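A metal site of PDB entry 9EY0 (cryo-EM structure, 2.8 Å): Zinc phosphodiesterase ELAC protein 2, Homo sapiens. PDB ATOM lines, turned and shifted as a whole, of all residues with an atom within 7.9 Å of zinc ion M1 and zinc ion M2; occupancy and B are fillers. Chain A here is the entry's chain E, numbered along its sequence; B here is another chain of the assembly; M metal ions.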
ATOM      1  N   GLY A 460     -18.620  26.106 -17.615  1.00  0.00           N
ATOM      2  CA  GLY A 460     -19.207  25.101 -18.472  1.00  0.00           C
ATOM      3  C   GLY A 460     -19.729  23.910 -17.698  1.00  0.00           C
ATOM      4  O   GLY A 460     -19.388  23.690 -16.540  1.00  0.00           O
ATOM      5  N   SER A 461     -20.564  23.115 -18.365  1.00  0.00           N
ATOM      6  CA  SER A 461     -21.185  21.950 -17.754  1.00  0.00           C
ATOM      7  C   SER A 461     -20.483  20.648 -18.153  1.00  0.00           C
ATOM      8  O   SER A 461     -19.977  19.929 -17.284  1.00  0.00           O
ATOM      9  CB  SER A 461     -22.678  21.880 -18.144  1.00  0.00           C
ATOM     10  OG  SER A 461     -22.835  21.849 -19.552  1.00  0.00           O
ATOM     11  N   ALA A 462     -20.454  20.336 -19.442  1.00  0.00           N
ATOM     12  CA  ALA A 462     -19.893  19.080 -19.921  1.00  0.00           C
ATOM     13  C   ALA A 462     -18.688  19.271 -20.836  1.00  0.00           C
ATOM     14  O   ALA A 462     -17.670  18.602 -20.637  1.00  0.00           O
ATOM     15  CB  ALA A 462     -20.980  18.285 -20.663  1.00  0.00           C
ATOM     16  N   VAL A 470     -15.213  24.626 -19.388  1.00  0.00           N
ATOM     17  CA  VAL A 470     -15.615  23.726 -18.324  1.00  0.00           C
ATOM     18  C   VAL A 470     -15.319  24.366 -16.965  1.00  0.00           C
ATOM     19  O   VAL A 470     -14.491  25.269 -16.840  1.00  0.00           O
ATOM     20  CB  VAL A 470     -14.916  22.358 -18.440  1.00  0.00           C
ATOM     21  CG1 VAL A 470     -15.516  21.562 -19.595  1.00  0.00           C
ATOM     22  CG2 VAL A 470     -13.421  22.534 -18.642  1.00  0.00           C
ATOM     23  N   SER A 471     -16.020  23.877 -15.940  1.00  0.00           N
ATOM     24  CA  SER A 471     -15.988  24.525 -14.637  1.00  0.00           C
ATOM     25  C   SER A 471     -14.562  24.614 -14.094  1.00  0.00           C
ATOM     26  O   SER A 471     -13.819  23.631 -14.086  1.00  0.00           O
ATOM     27  CB  SER A 471     -16.866  23.757 -13.652  1.00  0.00           C
ATOM     28  OG  SER A 471     -16.979  24.444 -12.418  1.00  0.00           O
ATOM     29  N   ASP A 486     -11.667  23.987  -8.820  1.00  0.00           N
ATOM     30  CA  ASP A 486     -11.918  22.946  -9.813  1.00  0.00           C
ATOM     31  C   ASP A 486     -10.933  23.139 -10.963  1.00  0.00           C
ATOM     32  O   ASP A 486     -10.474  24.253 -11.221  1.00  0.00           O
ATOM     33  CB  ASP A 486     -13.367  22.980 -10.314  1.00  0.00           C
ATOM     34  CG  ASP A 486     -14.188  21.809  -9.830  1.00  0.00           C
ATOM     35  OD1 ASP A 486     -15.422  21.953  -9.729  1.00  0.00           O
ATOM     36  OD2 ASP A 486     -13.612  20.742  -9.544  1.00  0.00           O
ATOM     37  N   SER A 516     -14.252  18.370  -7.222  1.00  0.00           N
ATOM     38  CA  SER A 516     -15.562  18.005  -6.695  1.00  0.00           C
ATOM     39  C   SER A 516     -15.822  16.518  -6.853  1.00  0.00           C
ATOM     40  O   SER A 516     -16.202  15.829  -5.885  1.00  0.00           O
ATOM     41  CB  SER A 516     -16.652  18.813  -7.389  1.00  0.00           C
ATOM     42  OG  SER A 516     -17.941  18.286  -7.121  1.00  0.00           O
ATOM     43  N   HIS A 517     -15.614  15.987  -8.049  1.00  0.00           N
ATOM     44  CA  HIS A 517     -15.810  14.565  -8.317  1.00  0.00           C
ATOM     45  C   HIS A 517     -14.991  14.189  -9.543  1.00  0.00           C
ATOM     46  O   HIS A 517     -14.174  14.972 -10.033  1.00  0.00           O
ATOM     47  CB  HIS A 517     -17.310  14.249  -8.475  1.00  0.00           C
ATOM     48  CG  HIS A 517     -18.013  15.113  -9.465  1.00  0.00           C
ATOM     49  ND1 HIS A 517     -18.133  16.475  -9.316  1.00  0.00           N
ATOM     50  CD2 HIS A 517     -18.650  14.803 -10.622  1.00  0.00           C
ATOM     51  CE1 HIS A 517     -18.805  16.977 -10.342  1.00  0.00           C
ATOM     52  NE2 HIS A 517     -19.134  15.977 -11.147  1.00  0.00           N
ATOM     53  N   LEU A 518     -15.228  12.983 -10.062  1.00  0.00           N
ATOM     54  CA  LEU A 518     -14.400  12.408 -11.118  1.00  0.00           C
ATOM     55  C   LEU A 518     -14.921  12.681 -12.518  1.00  0.00           C
ATOM     56  O   LEU A 518     -14.387  12.141 -13.484  1.00  0.00           O
ATOM     57  CB  LEU A 518     -14.263  10.893 -10.899  1.00  0.00           C
ATOM     58  CG  LEU A 518     -13.151  10.367  -9.977  1.00  0.00           C
ATOM     59  CD1 LEU A 518     -12.841   8.915 -10.308  1.00  0.00           C
ATOM     60  CD2 LEU A 518     -11.877  11.205 -10.049  1.00  0.00           C
ATOM     61  N   HIS A 519     -15.965  13.511 -12.653  1.00  0.00           N
ATOM     62  CA  HIS A 519     -16.442  13.866 -13.983  1.00  0.00           C
ATOM     63  C   HIS A 519     -15.325  14.529 -14.779  1.00  0.00           C
ATOM     64  O   HIS A 519     -14.540  15.319 -14.241  1.00  0.00           O
ATOM     65  CB  HIS A 519     -17.650  14.797 -13.884  1.00  0.00           C
ATOM     66  CG  HIS A 519     -18.957  14.070 -13.738  1.00  0.00           C
ATOM     67  ND1 HIS A 519     -20.117  14.708 -13.328  1.00  0.00           N
ATOM     68  CD2 HIS A 519     -19.296  12.775 -13.940  1.00  0.00           C
ATOM     69  CE1 HIS A 519     -21.106  13.837 -13.295  1.00  0.00           C
ATOM     70  NE2 HIS A 519     -20.630  12.654 -13.657  1.00  0.00           N
ATOM     71  N   ALA A 520     -15.263  14.216 -16.074  1.00  0.00           N
ATOM     72  CA  ALA A 520     -14.180  14.712 -16.909  1.00  0.00           C
ATOM     73  C   ALA A 520     -14.141  16.234 -16.931  1.00  0.00           C
ATOM     74  O   ALA A 520     -13.069  16.816 -17.146  1.00  0.00           O
ATOM     75  CB  ALA A 520     -14.307  14.162 -18.329  1.00  0.00           C
ATOM     76  N   ASP A 521     -15.277  16.891 -16.719  1.00  0.00           N
ATOM     77  CA  ASP A 521     -15.353  18.344 -16.751  1.00  0.00           C
ATOM     78  C   ASP A 521     -14.927  18.994 -15.440  1.00  0.00           C
ATOM     79  O   ASP A 521     -15.220  20.179 -15.241  1.00  0.00           O
ATOM     80  CB  ASP A 521     -16.773  18.791 -17.115  1.00  0.00           C
ATOM     81  CG  ASP A 521     -17.822  18.240 -16.160  1.00  0.00           C
ATOM     82  OD1 ASP A 521     -18.224  17.071 -16.326  1.00  0.00           O
ATOM     83  OD2 ASP A 521     -18.236  18.986 -15.246  1.00  0.00           O
ATOM     84  N   HIS A 522     -14.244  18.268 -14.557  1.00  0.00           N
ATOM     85  CA  HIS A 522     -13.814  18.815 -13.273  1.00  0.00           C
ATOM     86  C   HIS A 522     -12.374  18.501 -12.906  1.00  0.00           C
ATOM     87  O   HIS A 522     -11.826  19.187 -12.043  1.00  0.00           O
ATOM     88  CB  HIS A 522     -14.725  18.301 -12.145  1.00  0.00           C
ATOM     89  CG  HIS A 522     -16.144  18.772 -12.256  1.00  0.00           C
ATOM     90  ND1 HIS A 522     -16.618  19.865 -11.563  1.00  0.00           N
ATOM     91  CD2 HIS A 522     -17.180  18.286 -12.979  1.00  0.00           C
ATOM     92  CE1 HIS A 522     -17.894  20.037 -11.857  1.00  0.00           C
ATOM     93  NE2 HIS A 522     -18.268  19.097 -12.712  1.00  0.00           N
ATOM     94  N   HIS A 615     -24.994  13.732  -5.897  1.00  0.00           N
ATOM     95  CA  HIS A 615     -24.483  13.581  -7.255  1.00  0.00           C
ATOM     96  C   HIS A 615     -24.010  12.146  -7.415  1.00  0.00           C
ATOM     97  O   HIS A 615     -24.363  11.266  -6.618  1.00  0.00           O
ATOM     98  CB  HIS A 615     -23.391  14.631  -7.523  1.00  0.00           C
ATOM     99  CG  HIS A 615     -23.136  14.886  -8.985  1.00  0.00           C
ATOM    100  ND1 HIS A 615     -24.137  15.187  -9.863  1.00  0.00           N
ATOM    101  CD2 HIS A 615     -21.989  14.854  -9.701  1.00  0.00           C
ATOM    102  CE1 HIS A 615     -23.619  15.351 -11.075  1.00  0.00           C
ATOM    103  NE2 HIS A 615     -22.320  15.152 -11.000  1.00  0.00           N
ATOM    104  N   CYS A 616     -23.195  11.884  -8.441  1.00  0.00           N
ATOM    105  CA  CYS A 616     -22.635  10.560  -8.646  1.00  0.00           C
ATOM    106  C   CYS A 616     -21.842  10.127  -7.424  1.00  0.00           C
ATOM    107  O   CYS A 616     -21.532  10.942  -6.548  1.00  0.00           O
ATOM    108  CB  CYS A 616     -21.751  10.545  -9.895  1.00  0.00           C
ATOM    109  SG  CYS A 616     -20.254  11.548  -9.749  1.00  0.00           S
ATOM    110  N   ALA A 619     -18.931  12.001  -4.673  1.00  0.00           N
ATOM    111  CA  ALA A 619     -19.010  13.406  -5.035  1.00  0.00           C
ATOM    112  C   ALA A 619     -18.987  14.246  -3.757  1.00  0.00           C
ATOM    113  O   ALA A 619     -19.725  13.960  -2.813  1.00  0.00           O
ATOM    114  CB  ALA A 619     -20.271  13.705  -5.842  1.00  0.00           C
ATOM    115  N   TYR A 634     -18.366  26.356  -1.702  1.00  0.00           N
ATOM    116  CA  TYR A 634     -18.428  25.929  -3.091  1.00  0.00           C
ATOM    117  C   TYR A 634     -19.086  24.556  -3.160  1.00  0.00           C
ATOM    118  O   TYR A 634     -18.732  23.655  -2.403  1.00  0.00           O
ATOM    119  CB  TYR A 634     -17.030  25.868  -3.717  1.00  0.00           C
ATOM    120  CG  TYR A 634     -17.007  25.220  -5.085  1.00  0.00           C
ATOM    121  CD1 TYR A 634     -17.304  25.957  -6.221  1.00  0.00           C
ATOM    122  CD2 TYR A 634     -16.702  23.868  -5.233  1.00  0.00           C
ATOM    123  CE1 TYR A 634     -17.285  25.364  -7.478  1.00  0.00           C
ATOM    124  CE2 TYR A 634     -16.684  23.277  -6.481  1.00  0.00           C
ATOM    125  CZ  TYR A 634     -16.981  24.028  -7.600  1.00  0.00           C
ATOM    126  OH  TYR A 634     -16.965  23.439  -8.838  1.00  0.00           O
ATOM    127  N   GLY A 636     -20.015  21.578  -6.038  1.00  0.00           N
ATOM    128  CA  GLY A 636     -19.854  21.099  -7.397  1.00  0.00           C
ATOM    129  C   GLY A 636     -21.183  20.705  -8.002  1.00  0.00           C
ATOM    130  O   GLY A 636     -22.219  21.268  -7.641  1.00  0.00           O
ATOM    131  N   ASP A 637     -21.172  19.756  -8.930  1.00  0.00           N
ATOM    132  CA  ASP A 637     -22.418  19.242  -9.498  1.00  0.00           C
ATOM    133  C   ASP A 637     -23.222  18.576  -8.403  1.00  0.00           C
ATOM    134  O   ASP A 637     -22.767  17.601  -7.792  1.00  0.00           O
ATOM    135  CB  ASP A 637     -22.101  18.255 -10.627  1.00  0.00           C
ATOM    136  CG  ASP A 637     -21.181  18.844 -11.679  1.00  0.00           C
ATOM    137  OD1 ASP A 637     -20.912  20.062 -11.624  1.00  0.00           O
ATOM    138  OD2 ASP A 637     -20.735  18.082 -12.565  1.00  0.00           O
ATOM    139  N   THR A 638     -24.419  19.085  -8.123  1.00  0.00           N
ATOM    140  CA  THR A 638     -25.229  18.558  -7.041  1.00  0.00           C
ATOM    141  C   THR A 638     -26.683  18.991  -7.199  1.00  0.00           C
ATOM    142  O   THR A 638     -26.960  20.051  -7.766  1.00  0.00           O
ATOM    143  CB  THR A 638     -24.712  19.024  -5.676  1.00  0.00           C
ATOM    144  OG1 THR A 638     -25.571  18.519  -4.635  1.00  0.00           O
ATOM    145  CG2 THR A 638     -24.681  20.547  -5.596  1.00  0.00           C
ATOM    146  N   GLU A 657     -24.293  25.303  -8.319  1.00  0.00           N
ATOM    147  CA  GLU A 657     -24.577  24.925  -9.695  1.00  0.00           C
ATOM    148  C   GLU A 657     -25.963  25.416 -10.107  1.00  0.00           C
ATOM    149  O   GLU A 657     -26.918  25.347  -9.333  1.00  0.00           O
ATOM    150  CB  GLU A 657     -24.474  23.406  -9.852  1.00  0.00           C
ATOM    151  CG  GLU A 657     -25.235  22.823 -11.034  1.00  0.00           C
ATOM    152  CD  GLU A 657     -25.262  21.308 -11.012  1.00  0.00           C
ATOM    153  OE1 GLU A 657     -26.107  20.734 -10.315  1.00  0.00           O
ATOM    154  OE2 GLU A 657     -24.421  20.699 -11.707  1.00  0.00           O
ATOM    155  N   THR A 659     -27.162  24.515 -13.515  1.00  0.00           N
ATOM    156  CA  THR A 659     -27.034  23.943 -14.856  1.00  0.00           C
ATOM    157  C   THR A 659     -28.295  24.162 -15.686  1.00  0.00           C
ATOM    158  O   THR A 659     -28.219  24.625 -16.826  1.00  0.00           O
ATOM    159  CB  THR A 659     -26.722  22.443 -14.742  1.00  0.00           C
ATOM    160  OG1 THR A 659     -25.488  22.263 -14.039  1.00  0.00           O
ATOM    161  CG2 THR A 659     -26.601  21.822 -16.125  1.00  0.00           C
ATOM    162  N   LYS A 671     -30.436  13.834 -14.608  1.00  0.00           N
ATOM    163  CA  LYS A 671     -29.076  14.328 -14.807  1.00  0.00           C
ATOM    164  C   LYS A 671     -28.368  14.651 -13.500  1.00  0.00           C
ATOM    165  O   LYS A 671     -27.176  14.987 -13.530  1.00  0.00           O
ATOM    166  CB  LYS A 671     -29.112  15.578 -15.687  1.00  0.00           C
ATOM    167  CG  LYS A 671     -29.616  15.326 -17.099  1.00  0.00           C
ATOM    168  CD  LYS A 671     -29.805  16.628 -17.875  1.00  0.00           C
ATOM    169  CE  LYS A 671     -29.976  16.373 -19.358  1.00  0.00           C
ATOM    170  NZ  LYS A 671     -28.712  15.914 -20.002  1.00  0.00           N
ATOM    171  N   THR A 672     -29.056  14.544 -12.363  1.00  0.00           N
ATOM    172  CA  THR A 672     -28.463  14.812 -11.048  1.00  0.00           C
ATOM    173  C   THR A 672     -27.838  16.204 -10.997  1.00  0.00           C
ATOM    174  O   THR A 672     -26.632  16.379 -10.823  1.00  0.00           O
ATOM    175  CB  THR A 672     -27.441  13.735 -10.662  1.00  0.00           C
ATOM    176  OG1 THR A 672     -26.624  13.409 -11.797  1.00  0.00           O
ATOM    177  CG2 THR A 672     -28.141  12.481 -10.164  1.00  0.00           C
ATOM    178  N   HIS A 673     -28.690  17.219 -11.161  1.00  0.00           N
ATOM    179  CA  HIS A 673     -28.270  18.609 -11.106  1.00  0.00           C
ATOM    180  C   HIS A 673     -29.374  19.430 -10.472  1.00  0.00           C
ATOM    181  O   HIS A 673     -30.385  18.895 -10.002  1.00  0.00           O
ATOM    182  CB  HIS A 673     -27.911  19.130 -12.502  1.00  0.00           C
ATOM    183  CG  HIS A 673     -26.694  18.493 -13.092  1.00  0.00           C
ATOM    184  ND1 HIS A 673     -25.457  18.533 -12.479  1.00  0.00           N
ATOM    185  CD2 HIS A 673     -26.518  17.789 -14.242  1.00  0.00           C
ATOM    186  CE1 HIS A 673     -24.574  17.890 -13.223  1.00  0.00           C
ATOM    187  NE2 HIS A 673     -25.191  17.428 -14.291  1.00  0.00           N
ATOM    188  N   HIS A 695     -21.394  26.686 -13.540  1.00  0.00           N
ATOM    189  CA  HIS A 695     -21.623  25.352 -14.091  1.00  0.00           C
ATOM    190  C   HIS A 695     -22.899  25.317 -14.926  1.00  0.00           C
ATOM    191  O   HIS A 695     -23.671  24.362 -14.878  1.00  0.00           O
ATOM    192  CB  HIS A 695     -21.678  24.295 -12.978  1.00  0.00           C
ATOM    193  CG  HIS A 695     -21.406  22.905 -13.453  1.00  0.00           C
ATOM    194  ND1 HIS A 695     -22.389  22.084 -13.958  1.00  0.00           N
ATOM    195  CD2 HIS A 695     -20.256  22.185 -13.515  1.00  0.00           C
ATOM    196  CE1 HIS A 695     -21.868  20.922 -14.298  1.00  0.00           C
ATOM    197  NE2 HIS A 695     -20.572  20.962 -14.040  1.00  0.00           N
ATOM    198  P     C B  68     -25.932  19.230 -20.678  1.00  0.00           P
ATOM    199  OP1   C B  68     -27.318  18.741 -20.504  1.00  0.00           O
ATOM    200  OP2   C B  68     -25.641  20.688 -20.561  1.00  0.00           O
ATOM    201  O5'   C B  68     -25.007  18.460 -19.630  1.00  0.00           O
ATOM    202  C5'   C B  68     -25.303  18.495 -18.250  1.00  0.00           C
ATOM    203  C4'   C B  68     -25.157  17.125 -17.629  1.00  0.00           C
ATOM    204  O4'   C B  68     -25.912  16.155 -18.391  1.00  0.00           O
ATOM    205  C3'   C B  68     -23.747  16.547 -17.587  1.00  0.00           C
ATOM    206  O3'   C B  68     -22.964  17.058 -16.519  1.00  0.00           O
ATOM    207  C2'   C B  68     -24.006  15.051 -17.495  1.00  0.00           C
ATOM    208  O2'   C B  68     -24.319  14.664 -16.164  1.00  0.00           O
ATOM    209  C1'   C B  68     -25.256  14.903 -18.373  1.00  0.00           C
ATOM    210  N1    C B  68     -24.917  14.527 -19.764  1.00  0.00           N
ATOM    211  C2    C B  68     -24.678  13.182 -20.057  1.00  0.00           C
ATOM    212  O2    C B  68     -24.753  12.343 -19.141  1.00  0.00           O
ATOM    213  N3    C B  68     -24.371  12.819 -21.320  1.00  0.00           N
ATOM    214  C4    C B  68     -24.288  13.756 -22.278  1.00  0.00           C
ATOM    215  N4    C B  68     -23.987  13.357 -23.513  1.00  0.00           N
ATOM    216  C5    C B  68     -24.535  15.132 -22.004  1.00  0.00           C
ATOM    217  C6    C B  68     -24.839  15.471 -20.745  1.00  0.00           C
HETATM  218 ZN    ZN M   1     -19.810  19.068 -14.027  1.00  0.00          ZN
HETATM  219 ZN    ZN M   2     -20.918  16.141 -12.113  1.00  0.00          ZN
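ND1 of His 522 lies within hydrogen-bond range of OD1 of Asp 486. A ring nitrogen (ND1) of His 517 is in hydrogen-bond range of the side-chain hydroxyl (OG) of Ser 516, at 2.9 Å. NE2 of His 695 sits close to O of Ser 461, 3.5 Å away. ND1 of His 695 is in hydrogen-bond range of OE2 of Glu 657, 3.3 Å away. OG1 of Thr 659 lies within hydrogen-bond range of O of His 695 (2.9 Å). A ring nitrogen (ND1) of His 615 sits at hydrogen-bond distance from the backbone carbonyl oxygen (O) of Thr 672 (2.9 Å). The side-chain hydroxyl (OG) of Ser 461 is in hydrogen-bond range of OP2 of C 68 of chain B (3.2 Å).
Ser 461 touches zinc ion M1. Within 4 Å of zinc ion M1: Ser 461, Asp 521, His 522, Asp 637 and His 695. Along chain A the residues within 4 Å of zinc ion M1 span positions 461 to 695.
OD2 of Asp 637 binds zinc ion M1. OD2 of Asp 521 binds zinc ion M1 (2.0 Å). A ring nitrogen (NE2) of His 522 is bound to zinc ion M1 (2.0 Å). Zinc ion M1 is bound by a ring nitrogen (NE2) of His 695, at 2.0 Å. Slightly farther from zinc ion M1 lies OD1 of Asp 637 (2.8 Å).
Four residues have an atom within 4 Å of zinc ion M2: His 517, His 519, His 615 and Asp 637.
Zinc ion M2 is bound by OD2 of Asp 637, NE2 of His 517, ND1 of His 519 and NE2 of His 615. Zinc ion M2 has four donor atoms within binding distance.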
